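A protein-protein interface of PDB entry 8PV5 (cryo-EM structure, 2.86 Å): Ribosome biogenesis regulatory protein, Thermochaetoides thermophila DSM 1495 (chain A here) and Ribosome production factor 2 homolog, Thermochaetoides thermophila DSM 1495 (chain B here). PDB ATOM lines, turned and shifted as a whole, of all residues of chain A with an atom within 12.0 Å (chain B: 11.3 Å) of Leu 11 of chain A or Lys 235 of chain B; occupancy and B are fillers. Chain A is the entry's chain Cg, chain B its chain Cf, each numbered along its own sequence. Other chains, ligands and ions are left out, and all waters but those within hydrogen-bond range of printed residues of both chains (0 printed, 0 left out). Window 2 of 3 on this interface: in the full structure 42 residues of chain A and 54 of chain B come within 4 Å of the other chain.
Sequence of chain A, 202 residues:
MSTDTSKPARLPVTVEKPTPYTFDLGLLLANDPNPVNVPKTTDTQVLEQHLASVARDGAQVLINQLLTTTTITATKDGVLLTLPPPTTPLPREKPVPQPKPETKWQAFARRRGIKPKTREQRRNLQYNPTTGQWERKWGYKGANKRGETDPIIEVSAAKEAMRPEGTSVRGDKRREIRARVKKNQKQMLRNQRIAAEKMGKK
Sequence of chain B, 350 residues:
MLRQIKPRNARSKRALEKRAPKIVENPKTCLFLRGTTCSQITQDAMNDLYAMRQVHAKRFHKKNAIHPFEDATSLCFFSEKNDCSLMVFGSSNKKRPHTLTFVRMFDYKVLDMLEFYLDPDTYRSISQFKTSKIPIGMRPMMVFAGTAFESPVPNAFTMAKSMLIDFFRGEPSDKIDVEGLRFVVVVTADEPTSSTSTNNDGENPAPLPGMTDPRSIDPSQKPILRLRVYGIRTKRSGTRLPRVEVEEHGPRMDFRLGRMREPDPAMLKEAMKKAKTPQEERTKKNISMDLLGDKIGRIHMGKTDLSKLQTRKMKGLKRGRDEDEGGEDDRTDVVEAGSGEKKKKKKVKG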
ATOM      1  N   LEU A  11     -22.186   7.297 -29.619  1.00  0.00           N
ATOM      2  CA  LEU A  11     -22.254   7.033 -28.186  1.00  0.00           C
ATOM      3  C   LEU A  11     -21.410   8.034 -27.392  1.00  0.00           C
ATOM      4  O   LEU A  11     -20.272   8.331 -27.759  1.00  0.00           O
ATOM      5  CB  LEU A  11     -21.846   5.578 -27.902  1.00  0.00           C
ATOM      6  CG  LEU A  11     -20.476   4.991 -28.273  1.00  0.00           C
ATOM      7  CD1 LEU A  11     -19.393   5.248 -27.235  1.00  0.00           C
ATOM      8  CD2 LEU A  11     -20.609   3.498 -28.543  1.00  0.00           C
ATOM      9  N   PRO A  12     -21.984   8.576 -26.320  1.00  0.00           N
ATOM     10  CA  PRO A  12     -21.305   9.643 -25.579  1.00  0.00           C
ATOM     11  C   PRO A  12     -20.223   9.110 -24.655  1.00  0.00           C
ATOM     12  O   PRO A  12     -20.176   7.923 -24.325  1.00  0.00           O
ATOM     13  CB  PRO A  12     -22.442  10.286 -24.779  1.00  0.00           C
ATOM     14  CG  PRO A  12     -23.380   9.151 -24.538  1.00  0.00           C
ATOM     15  CD  PRO A  12     -23.341   8.326 -25.800  1.00  0.00           C
ATOM     16  N   VAL A  13     -19.344  10.018 -24.239  1.00  0.00           N
ATOM     17  CA  VAL A  13     -18.340   9.739 -23.223  1.00  0.00           C
ATOM     18  C   VAL A  13     -18.605  10.547 -21.953  1.00  0.00           C
ATOM     19  O   VAL A  13     -17.770  10.583 -21.054  1.00  0.00           O
ATOM     20  CB  VAL A  13     -16.921   9.993 -23.755  1.00  0.00           C
ATOM     21  CG1 VAL A  13     -16.595   9.021 -24.873  1.00  0.00           C
ATOM     22  CG2 VAL A  13     -16.786  11.429 -24.232  1.00  0.00           C
ATOM     23  N   THR A  14     -19.762  11.202 -21.874  1.00  0.00           N
ATOM     24  CA  THR A  14     -20.135  12.013 -20.727  1.00  0.00           C
ATOM     25  C   THR A  14     -21.493  11.558 -20.212  1.00  0.00           C
ATOM     26  O   THR A  14     -22.421  11.321 -20.991  1.00  0.00           O
ATOM     27  CB  THR A  14     -20.182  13.506 -21.088  1.00  0.00           C
ATOM     28  OG1 THR A  14     -18.997  13.860 -21.811  1.00  0.00           O
ATOM     29  CG2 THR A  14     -20.273  14.364 -19.835  1.00  0.00           C
ATOM     30  N   VAL A  15     -21.602  11.439 -18.892  1.00  0.00           N
ATOM     31  CA  VAL A  15     -22.813  10.958 -18.241  1.00  0.00           C
ATOM     32  C   VAL A  15     -23.497  12.126 -17.546  1.00  0.00           C
ATOM     33  O   VAL A  15     -22.883  13.174 -17.320  1.00  0.00           O
ATOM     34  CB  VAL A  15     -22.510   9.825 -17.239  1.00  0.00           C
ATOM     35  CG1 VAL A  15     -21.684   8.740 -17.907  1.00  0.00           C
ATOM     36  CG2 VAL A  15     -21.794  10.370 -16.015  1.00  0.00           C
ATOM     37  N   GLU A  16     -24.775  11.946 -17.225  1.00  0.00           N
ATOM     38  CA  GLU A  16     -25.568  12.950 -16.530  1.00  0.00           C
ATOM     39  C   GLU A  16     -26.204  12.322 -15.299  1.00  0.00           C
ATOM     40  O   GLU A  16     -26.868  11.284 -15.398  1.00  0.00           O
ATOM     41  CB  GLU A  16     -26.649  13.532 -17.449  1.00  0.00           C
ATOM     42  CG  GLU A  16     -27.500  14.625 -16.811  1.00  0.00           C
ATOM     43  CD  GLU A  16     -26.713  15.879 -16.470  1.00  0.00           C
ATOM     44  OE1 GLU A  16     -25.677  16.143 -17.117  1.00  0.00           O
ATOM     45  OE2 GLU A  16     -27.134  16.606 -15.545  1.00  0.00           O
ATOM     46  N   ARG A  56     -18.755   1.592 -14.650  1.00  0.00           N
ATOM     47  CA  ARG A  56     -18.318   2.166 -15.915  1.00  0.00           C
ATOM     48  C   ARG A  56     -18.490   3.676 -15.917  1.00  0.00           C
ATOM     49  O   ARG A  56     -17.622   4.402 -16.411  1.00  0.00           O
ATOM     50  CB  ARG A  56     -19.101   1.529 -17.062  1.00  0.00           C
ATOM     51  CG  ARG A  56     -18.454   1.644 -18.429  1.00  0.00           C
ATOM     52  CD  ARG A  56     -19.418   2.218 -19.452  1.00  0.00           C
ATOM     53  NE  ARG A  56     -20.105   3.406 -18.964  1.00  0.00           N
ATOM     54  CZ  ARG A  56     -19.665   4.644 -19.139  1.00  0.00           C
ATOM     55  NH1 ARG A  56     -18.546   4.892 -19.800  1.00  0.00           N
ATOM     56  NH2 ARG A  56     -20.368   5.659 -18.646  1.00  0.00           N
ATOM     57  N   ASP A  57     -19.598   4.166 -15.353  1.00  0.00           N
ATOM     58  CA  ASP A  57     -19.806   5.608 -15.247  1.00  0.00           C
ATOM     59  C   ASP A  57     -18.748   6.253 -14.355  1.00  0.00           C
ATOM     60  O   ASP A  57     -18.179   7.300 -14.699  1.00  0.00           O
ATOM     61  CB  ASP A  57     -21.207   5.891 -14.708  1.00  0.00           C
ATOM     62  CG  ASP A  57     -22.296   5.522 -15.694  1.00  0.00           C
ATOM     63  OD1 ASP A  57     -22.039   5.581 -16.914  1.00  0.00           O
ATOM     64  OD2 ASP A  57     -23.409   5.172 -15.249  1.00  0.00           O
ATOM     65  N   ALA A  59     -15.688   5.059 -13.572  1.00  0.00           N
ATOM     66  CA  ALA A  59     -14.391   4.986 -14.234  1.00  0.00           C
ATOM     67  C   ALA A  59     -14.294   5.992 -15.372  1.00  0.00           C
ATOM     68  O   ALA A  59     -13.244   6.612 -15.568  1.00  0.00           O
ATOM     69  CB  ALA A  59     -14.141   3.569 -14.747  1.00  0.00           C
ATOM     70  N   GLN A  60     -15.387   6.181 -16.118  1.00  0.00           N
ATOM     71  CA  GLN A  60     -15.392   7.135 -17.221  1.00  0.00           C
ATOM     72  C   GLN A  60     -15.165   8.556 -16.726  1.00  0.00           C
ATOM     73  O   GLN A  60     -14.312   9.276 -17.258  1.00  0.00           O
ATOM     74  CB  GLN A  60     -16.714   7.041 -17.983  1.00  0.00           C
ATOM     75  CG  GLN A  60     -16.852   8.043 -19.114  1.00  0.00           C
ATOM     76  CD  GLN A  60     -16.104   7.621 -20.360  1.00  0.00           C
ATOM     77  OE1 GLN A  60     -16.331   6.538 -20.896  1.00  0.00           O
ATOM     78  NE2 GLN A  60     -15.202   8.477 -20.827  1.00  0.00           N
ATOM     79  N   ILE A  63     -11.465   8.921 -15.395  1.00  0.00           N
ATOM     80  CA  ILE A  63     -10.469   9.059 -16.460  1.00  0.00           C
ATOM     81  C   ILE A  63     -10.620  10.402 -17.170  1.00  0.00           C
ATOM     82  O   ILE A  63      -9.622  11.027 -17.554  1.00  0.00           O
ATOM     83  CB  ILE A  63     -10.551   7.871 -17.442  1.00  0.00           C
ATOM     84  CG1 ILE A  63     -10.305   6.551 -16.712  1.00  0.00           C
ATOM     85  CG2 ILE A  63      -9.541   8.006 -18.572  1.00  0.00           C
ATOM     86  CD1 ILE A  63      -8.943   6.454 -16.065  1.00  0.00           C
ATOM     87  N   ASN A  64     -11.859  10.878 -17.341  1.00  0.00           N
ATOM     88  CA  ASN A  64     -12.062  12.199 -17.932  1.00  0.00           C
ATOM     89  C   ASN A  64     -11.464  13.299 -17.063  1.00  0.00           C
ATOM     90  O   ASN A  64     -10.809  14.215 -17.576  1.00  0.00           O
ATOM     91  CB  ASN A  64     -13.552  12.455 -18.166  1.00  0.00           C
ATOM     92  CG  ASN A  64     -14.126  11.593 -19.270  1.00  0.00           C
ATOM     93  OD1 ASN A  64     -13.393  11.047 -20.092  1.00  0.00           O
ATOM     94  ND2 ASN A  64     -15.446  11.464 -19.291  1.00  0.00           N
ATOM     95  N   LEU A  67      -7.629  13.124 -17.373  1.00  0.00           N
ATOM     96  CA  LEU A  67      -7.132  13.618 -18.649  1.00  0.00           C
ATOM     97  C   LEU A  67      -7.431  15.092 -18.883  1.00  0.00           C
ATOM     98  O   LEU A  67      -6.831  15.687 -19.783  1.00  0.00           O
ATOM     99  CB  LEU A  67      -7.713  12.793 -19.798  1.00  0.00           C
ATOM    100  CG  LEU A  67      -7.213  11.352 -19.910  1.00  0.00           C
ATOM    101  CD1 LEU A  67      -7.773  10.690 -21.154  1.00  0.00           C
ATOM    102  CD2 LEU A  67      -5.696  11.299 -19.911  1.00  0.00           C
ATOM    103  N   LEU B 181      -3.819   3.120 -15.412  1.00  0.00           N
ATOM    104  CA  LEU B 181      -5.188   3.525 -15.097  1.00  0.00           C
ATOM    105  C   LEU B 181      -6.136   2.479 -15.687  1.00  0.00           C
ATOM    106  O   LEU B 181      -7.118   2.809 -16.355  1.00  0.00           O
ATOM    107  CB  LEU B 181      -5.493   4.923 -15.637  1.00  0.00           C
ATOM    108  CG  LEU B 181      -4.519   6.057 -15.311  1.00  0.00           C
ATOM    109  CD1 LEU B 181      -4.880   7.313 -16.090  1.00  0.00           C
ATOM    110  CD2 LEU B 181      -4.479   6.340 -13.820  1.00  0.00           C
ATOM    111  N   ARG B 182      -5.831   1.207 -15.442  1.00  0.00           N
ATOM    112  CA  ARG B 182      -6.526   0.111 -16.100  1.00  0.00           C
ATOM    113  C   ARG B 182      -7.300  -0.814 -15.166  1.00  0.00           C
ATOM    114  O   ARG B 182      -7.954  -1.742 -15.657  1.00  0.00           O
ATOM    115  CB  ARG B 182      -5.526  -0.701 -16.938  1.00  0.00           C
ATOM    116  CG  ARG B 182      -4.490  -1.443 -16.122  1.00  0.00           C
ATOM    117  CD  ARG B 182      -3.517  -2.232 -16.986  1.00  0.00           C
ATOM    118  NE  ARG B 182      -2.676  -1.376 -17.813  1.00  0.00           N
ATOM    119  CZ  ARG B 182      -2.791  -1.261 -19.129  1.00  0.00           C
ATOM    120  NH1 ARG B 182      -3.707  -1.936 -19.802  1.00  0.00           N
ATOM    121  NH2 ARG B 182      -1.964  -0.452 -19.783  1.00  0.00           N
ATOM    122  N   GLY B 231     -11.644  -4.451 -14.776  1.00  0.00           N
ATOM    123  CA  GLY B 231     -10.613  -3.984 -15.678  1.00  0.00           C
ATOM    124  C   GLY B 231     -11.191  -3.015 -16.693  1.00  0.00           C
ATOM    125  O   GLY B 231     -12.374  -3.058 -17.013  1.00  0.00           O
ATOM    126  N   ILE B 232     -10.339  -2.132 -17.206  1.00  0.00           N
ATOM    127  CA  ILE B 232     -10.779  -0.996 -18.006  1.00  0.00           C
ATOM    128  C   ILE B 232     -10.256  -1.121 -19.429  1.00  0.00           C
ATOM    129  O   ILE B 232      -9.052  -1.300 -19.651  1.00  0.00           O
ATOM    130  CB  ILE B 232     -10.330   0.332 -17.366  1.00  0.00           C
ATOM    131  CG1 ILE B 232     -11.061   0.535 -16.041  1.00  0.00           C
ATOM    132  CG2 ILE B 232     -10.568   1.502 -18.303  1.00  0.00           C
ATOM    133  CD1 ILE B 232     -10.584   1.718 -15.268  1.00  0.00           C
ATOM    134  N   ARG B 233     -11.170  -1.024 -20.392  1.00  0.00           N
ATOM    135  CA  ARG B 233     -10.846  -0.964 -21.807  1.00  0.00           C
ATOM    136  C   ARG B 233     -11.225   0.409 -22.346  1.00  0.00           C
ATOM    137  O   ARG B 233     -12.215   1.008 -21.918  1.00  0.00           O
ATOM    138  CB  ARG B 233     -11.584  -2.051 -22.597  1.00  0.00           C
ATOM    139  CG  ARG B 233     -11.234  -3.472 -22.193  1.00  0.00           C
ATOM    140  CD  ARG B 233      -9.807  -3.825 -22.573  1.00  0.00           C
ATOM    141  NE  ARG B 233      -9.485  -5.210 -22.253  1.00  0.00           N
ATOM    142  CZ  ARG B 233      -8.289  -5.758 -22.416  1.00  0.00           C
ATOM    143  NH1 ARG B 233      -7.270  -5.063 -22.894  1.00  0.00           N
ATOM    144  NH2 ARG B 233      -8.110  -7.036 -22.090  1.00  0.00           N
ATOM    145  N   THR B 234     -10.429   0.905 -23.289  1.00  0.00           N
ATOM    146  CA  THR B 234     -10.649   2.209 -23.898  1.00  0.00           C
ATOM    147  C   THR B 234     -10.910   2.042 -25.388  1.00  0.00           C
ATOM    148  O   THR B 234     -10.233   1.262 -26.063  1.00  0.00           O
ATOM    149  CB  THR B 234      -9.453   3.137 -23.676  1.00  0.00           C
ATOM    150  OG1 THR B 234      -8.267   2.523 -24.195  1.00  0.00           O
ATOM    151  CG2 THR B 234      -9.266   3.417 -22.194  1.00  0.00           C
ATOM    152  N   LYS B 235     -11.896   2.780 -25.894  1.00  0.00           N
ATOM    153  CA  LYS B 235     -12.349   2.653 -27.270  1.00  0.00           C
ATOM    154  C   LYS B 235     -12.487   4.042 -27.883  1.00  0.00           C
ATOM    155  O   LYS B 235     -12.811   5.014 -27.195  1.00  0.00           O
ATOM    156  CB  LYS B 235     -13.684   1.883 -27.330  1.00  0.00           C
ATOM    157  CG  LYS B 235     -14.243   1.630 -28.723  1.00  0.00           C
ATOM    158  CD  LYS B 235     -15.478   0.747 -28.672  1.00  0.00           C
ATOM    159  CE  LYS B 235     -16.668   1.496 -28.098  1.00  0.00           C
ATOM    160  NZ  LYS B 235     -17.134   2.573 -29.014  1.00  0.00           N
ATOM    161  N   ARG B 236     -12.218   4.129 -29.187  1.00  0.00           N
ATOM    162  CA  ARG B 236     -12.382   5.382 -29.914  1.00  0.00           C
ATOM    163  C   ARG B 236     -13.848   5.790 -29.950  1.00  0.00           C
ATOM    164  O   ARG B 236     -14.736   4.946 -30.101  1.00  0.00           O
ATOM    165  CB  ARG B 236     -11.851   5.248 -31.341  1.00  0.00           C
ATOM    166  CG  ARG B 236     -10.403   4.824 -31.441  1.00  0.00           C
ATOM    167  CD  ARG B 236      -9.887   4.946 -32.862  1.00  0.00           C
ATOM    168  NE  ARG B 236      -8.477   4.591 -32.954  1.00  0.00           N
ATOM    169  CZ  ARG B 236      -7.476   5.428 -32.723  1.00  0.00           C
ATOM    170  NH1 ARG B 236      -7.695   6.687 -32.378  1.00  0.00           N
ATOM    171  NH2 ARG B 236      -6.225   4.994 -32.840  1.00  0.00           N
ATOM    172  N   SER B 237     -14.101   7.092 -29.808  1.00  0.00           N
ATOM    173  CA  SER B 237     -15.455   7.629 -29.829  1.00  0.00           C
ATOM    174  C   SER B 237     -15.592   8.841 -30.742  1.00  0.00           C
ATOM    175  O   SER B 237     -16.624   9.519 -30.701  1.00  0.00           O
ATOM    176  CB  SER B 237     -15.900   7.995 -28.411  1.00  0.00           C
ATOM    177  OG  SER B 237     -15.193   9.127 -27.935  1.00  0.00           O
ATOM    178  N   GLY B 238     -14.582   9.136 -31.559  1.00  0.00           N
ATOM    179  CA  GLY B 238     -14.600  10.331 -32.377  1.00  0.00           C
ATOM    180  C   GLY B 238     -14.334  11.615 -31.627  1.00  0.00           C
ATOM    181  O   GLY B 238     -14.506  12.697 -32.200  1.00  0.00           O
ATOM    182  N   THR B 239     -13.922  11.529 -30.366  1.00  0.00           N
ATOM    183  CA  THR B 239     -13.683  12.667 -29.495  1.00  0.00           C
ATOM    184  C   THR B 239     -12.344  12.421 -28.799  1.00  0.00           C
ATOM    185  O   THR B 239     -11.872  11.281 -28.727  1.00  0.00           O
ATOM    186  CB  THR B 239     -14.857  12.831 -28.512  1.00  0.00           C
ATOM    187  OG1 THR B 239     -16.083  12.862 -29.252  1.00  0.00           O
ATOM    188  CG2 THR B 239     -14.777  14.136 -27.720  1.00  0.00           C
ATOM    189  N   ARG B 240     -11.705  13.497 -28.328  1.00  0.00           N
ATOM    190  CA  ARG B 240     -10.416  13.379 -27.649  1.00  0.00           C
ATOM    191  C   ARG B 240     -10.525  12.518 -26.394  1.00  0.00           C
ATOM    192  O   ARG B 240      -9.638  11.706 -26.106  1.00  0.00           O
ATOM    193  CB  ARG B 240      -9.881  14.769 -27.305  1.00  0.00           C
ATOM    194  CG  ARG B 240      -8.539  14.762 -26.593  1.00  0.00           C
ATOM    195  CD  ARG B 240      -8.053  16.174 -26.314  1.00  0.00           C
ATOM    196  NE  ARG B 240      -6.774  16.180 -25.616  1.00  0.00           N
ATOM    197  CZ  ARG B 240      -6.643  16.165 -24.296  1.00  0.00           C
ATOM    198  NH1 ARG B 240      -7.696  16.140 -23.497  1.00  0.00           N
ATOM    199  NH2 ARG B 240      -5.423  16.176 -23.766  1.00  0.00           N
ATOM    200  N   LEU B 241     -11.607  12.677 -25.640  1.00  0.00           N
ATOM    201  CA  LEU B 241     -11.816  11.839 -24.470  1.00  0.00           C
ATOM    202  C   LEU B 241     -12.214  10.428 -24.897  1.00  0.00           C
ATOM    203  O   LEU B 241     -13.169  10.255 -25.661  1.00  0.00           O
ATOM    204  CB  LEU B 241     -12.892  12.436 -23.567  1.00  0.00           C
ATOM    205  CG  LEU B 241     -12.492  13.707 -22.818  1.00  0.00           C
ATOM    206  CD1 LEU B 241     -13.653  14.227 -21.985  1.00  0.00           C
ATOM    207  CD2 LEU B 241     -11.270  13.456 -21.951  1.00  0.00           C
ATOM    208  N   PRO B 242     -11.504   9.405 -24.431  1.00  0.00           N
ATOM    209  CA  PRO B 242     -11.831   8.031 -24.820  1.00  0.00           C
ATOM    210  C   PRO B 242     -13.086   7.525 -24.128  1.00  0.00           C
ATOM    211  O   PRO B 242     -13.563   8.090 -23.141  1.00  0.00           O
ATOM    212  CB  PRO B 242     -10.601   7.237 -24.369  1.00  0.00           C
ATOM    213  CG  PRO B 242     -10.073   8.017 -23.220  1.00  0.00           C
ATOM    214  CD  PRO B 242     -10.332   9.462 -23.542  1.00  0.00           C
ATOM    215  N   ARG B 243     -13.622   6.437 -24.671  1.00  0.00           N
ATOM    216  CA  ARG B 243     -14.797   5.787 -24.107  1.00  0.00           C
ATOM    217  C   ARG B 243     -14.346   4.620 -23.238  1.00  0.00           C
ATOM    218  O   ARG B 243     -13.672   3.703 -23.720  1.00  0.00           O
ATOM    219  CB  ARG B 243     -15.740   5.311 -25.209  1.00  0.00           C
ATOM    220  CG  ARG B 243     -16.760   4.280 -24.754  1.00  0.00           C
ATOM    221  CD  ARG B 243     -17.862   4.923 -23.926  1.00  0.00           C
ATOM    222  NE  ARG B 243     -18.911   3.970 -23.580  1.00  0.00           N
ATOM    223  CZ  ARG B 243     -20.066   4.301 -23.021  1.00  0.00           C
ATOM    224  NH1 ARG B 243     -20.358   5.557 -22.729  1.00  0.00           N
ATOM    225  NH2 ARG B 243     -20.952   3.347 -22.751  1.00  0.00           N
ATOM    226  N   VAL B 244     -14.718   4.658 -21.967  1.00  0.00           N
ATOM    227  CA  VAL B 244     -14.281   3.654 -21.005  1.00  0.00           C
ATOM    228  C   VAL B 244     -15.270   2.499 -20.991  1.00  0.00           C
ATOM    229  O   VAL B 244     -16.481   2.698 -20.838  1.00  0.00           O
ATOM    230  CB  VAL B 244     -14.131   4.285 -19.609  1.00  0.00           C
ATOM    231  CG1 VAL B 244     -13.849   3.218 -18.569  1.00  0.00           C
ATOM    232  CG2 VAL B 244     -13.027   5.327 -19.620  1.00  0.00           C
ATOM    233  N   GLU B 245     -14.756   1.284 -21.164  1.00  0.00           N
ATOM    234  CA  GLU B 245     -15.556   0.073 -21.071  1.00  0.00           C
ATOM    235  C   GLU B 245     -14.954  -0.828 -20.005  1.00  0.00           C
ATOM    236  O   GLU B 245     -13.731  -0.952 -19.899  1.00  0.00           O
ATOM    237  CB  GLU B 245     -15.630  -0.664 -22.414  1.00  0.00           C
ATOM    238  CG  GLU B 245     -16.323   0.120 -23.517  1.00  0.00           C
ATOM    239  CD  GLU B 245     -17.827   0.178 -23.339  1.00  0.00           C
ATOM    240  OE1 GLU B 245     -18.382  -0.695 -22.639  1.00  0.00           O
ATOM    241  OE2 GLU B 245     -18.457   1.098 -23.902  1.00  0.00           O
ATOM    242  N   VAL B 246     -15.819  -1.459 -19.215  1.00  0.00           N
ATOM    243  CA  VAL B 246     -15.380  -2.239 -18.068  1.00  0.00           C
ATOM    244  C   VAL B 246     -15.600  -3.721 -18.334  1.00  0.00           C
ATOM    245  O   VAL B 246     -16.489  -4.126 -19.086  1.00  0.00           O
ATOM    246  CB  VAL B 246     -16.089  -1.818 -16.765  1.00  0.00           C
ATOM    247  CG1 VAL B 246     -15.622  -0.440 -16.329  1.00  0.00           C
ATOM    248  CG2 VAL B 246     -17.596  -1.854 -16.943  1.00  0.00           C
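Among the printed residues, merely in contact across the chains: Val 13 of chain A with Ser 237 of chain B (3.4 Å), Arg 56 of chain A with Arg 243 of chain B (3.5 Å), Val 13 of chain A with Pro 242 of chain B (3.6 Å), Gln 60 of chain A with Arg 243 of chain B (3.6 Å), Leu 11 of chain A with Lys 235 of chain B (3.6 Å), Leu 11 of chain A with Arg 243 of chain B (3.7 Å), Arg 56 of chain A with Val 246 of chain B (3.7 Å), Leu 67 of chain A with Pro 242 of chain B (3.7 Å), Asn 64 of chain A with Leu 241 of chain B (3.7 Å), Val 13 of chain A with Leu 241 of chain B (3.7 Å), Val 13 of chain A with Arg 243 of chain B (3.8 Å), Ile 63 of chain A with Leu 181 of chain B (3.8 Å), Leu 67 of chain A with Arg 240 of chain B (3.8 Å) and Ala 59 of chain A with Val 244 of chain B (3.8 Å).
O of Val 13 of chain A lies close to NE2 of Gln 60 of chain A, at 3.3 Å. OD1 of Asp 57 of chain A lies within salt-bridge range of NH2 of Arg 56 of chain A, at 2.4 Å. The backbone carbonyl oxygen (O) of Arg 243 of chain B is in hydrogen-bond range of the backbone NH (N) of Lys 235 of chain B, 3.0 Å away. NH1 of Arg 56 of chain A is in hydrogen-bond range of OE1 of Gln 60 of chain A (3.0 Å). O of Val 13 of chain A sits at hydrogen-bond distance from ND2 of Asn 64 of chain A, 3.0 Å away. The side-chain hydroxyl (OG) of Ser 237 of chain B is in hydrogen-bond range of the backbone carbonyl oxygen (O) of Leu 241 of chain B.
Of the 13 printed residues of chain A, 9 touch a printed residue of chain B. Printed residues of chain A that touch a printed residue of chain B: Leu 11, Pro 12, Val 13, Arg 56, Ala 59, Gln 60, Ile 63, Asn 64 and Leu 67. Hydrophobic or aromatic side chains of chain A within 4 Å of the printed part of chain B: Leu 11, Val 13, Ala 59, Ile 63 and Leu 67. Printed residues of chain B that touch a printed residue of chain A: Leu 181, Lys 235, Ser 237, Arg 240, Leu 241, Pro 242, Arg 243, Val 244 and Val 246. Among the printed residues, 18 pairs touch across the chains. Among the printed residues, no Asp or Glu carboxylate lies within 4 Å of a Lys or Arg side-chain nitrogen of the other chain.
N of Val 244 of chain B is in hydrogen-bond range of OE1 of Gln 60 of chain A, 2.7 Å away. The guanidinium group of Arg 243 of chain B is in hydrogen-bond range of the backbone carbonyl oxygen of Pro 12 of chain A. O of Val 244 of chain B lies within hydrogen-bond range of NH1 of Arg 56 of chain A (3.2 Å). The side-chain amide nitrogen (NE2) of Gln 60 of chain A sits at hydrogen-bond distance from the backbone carbonyl oxygen (O) of Pro 242 of chain B.
Leu 11 of chain A touches just these residues of chain B: Lys 235 (3.6 Å) and Arg 243 (3.7 Å). Of the printed residues of chain B, Ala 59 of chain A touches Val 244. Arg 233 of chain B touches none of the printed residues of chain A. No residue of chain A comes within 4 Å of Thr 234 of chain B. Of the printed residues of chain A, Lys 235 of chain B touches Leu 11 (3.6 Å). Of chain A, only Val 13 (3.4 Å) comes within 4 Å of Ser 237 of chain B. Gly 238 of chain B touches none of the printed residues of chain A. Printed residues of chain A within 4 Å of Arg 240 of chain B: Leu 67 (3.8 Å). Of chain A, only Leu 11, Pro 12, Val 13, Arg 56 and Gln 60 come within 4 Å of Arg 243 of chain B. Of the printed residues of chain A, Val 246 of chain B touches Arg 56. The nearest printed residue of chain A that does not touch Val 246 of chain B is Ala 59 of chain A (4.6 Å).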
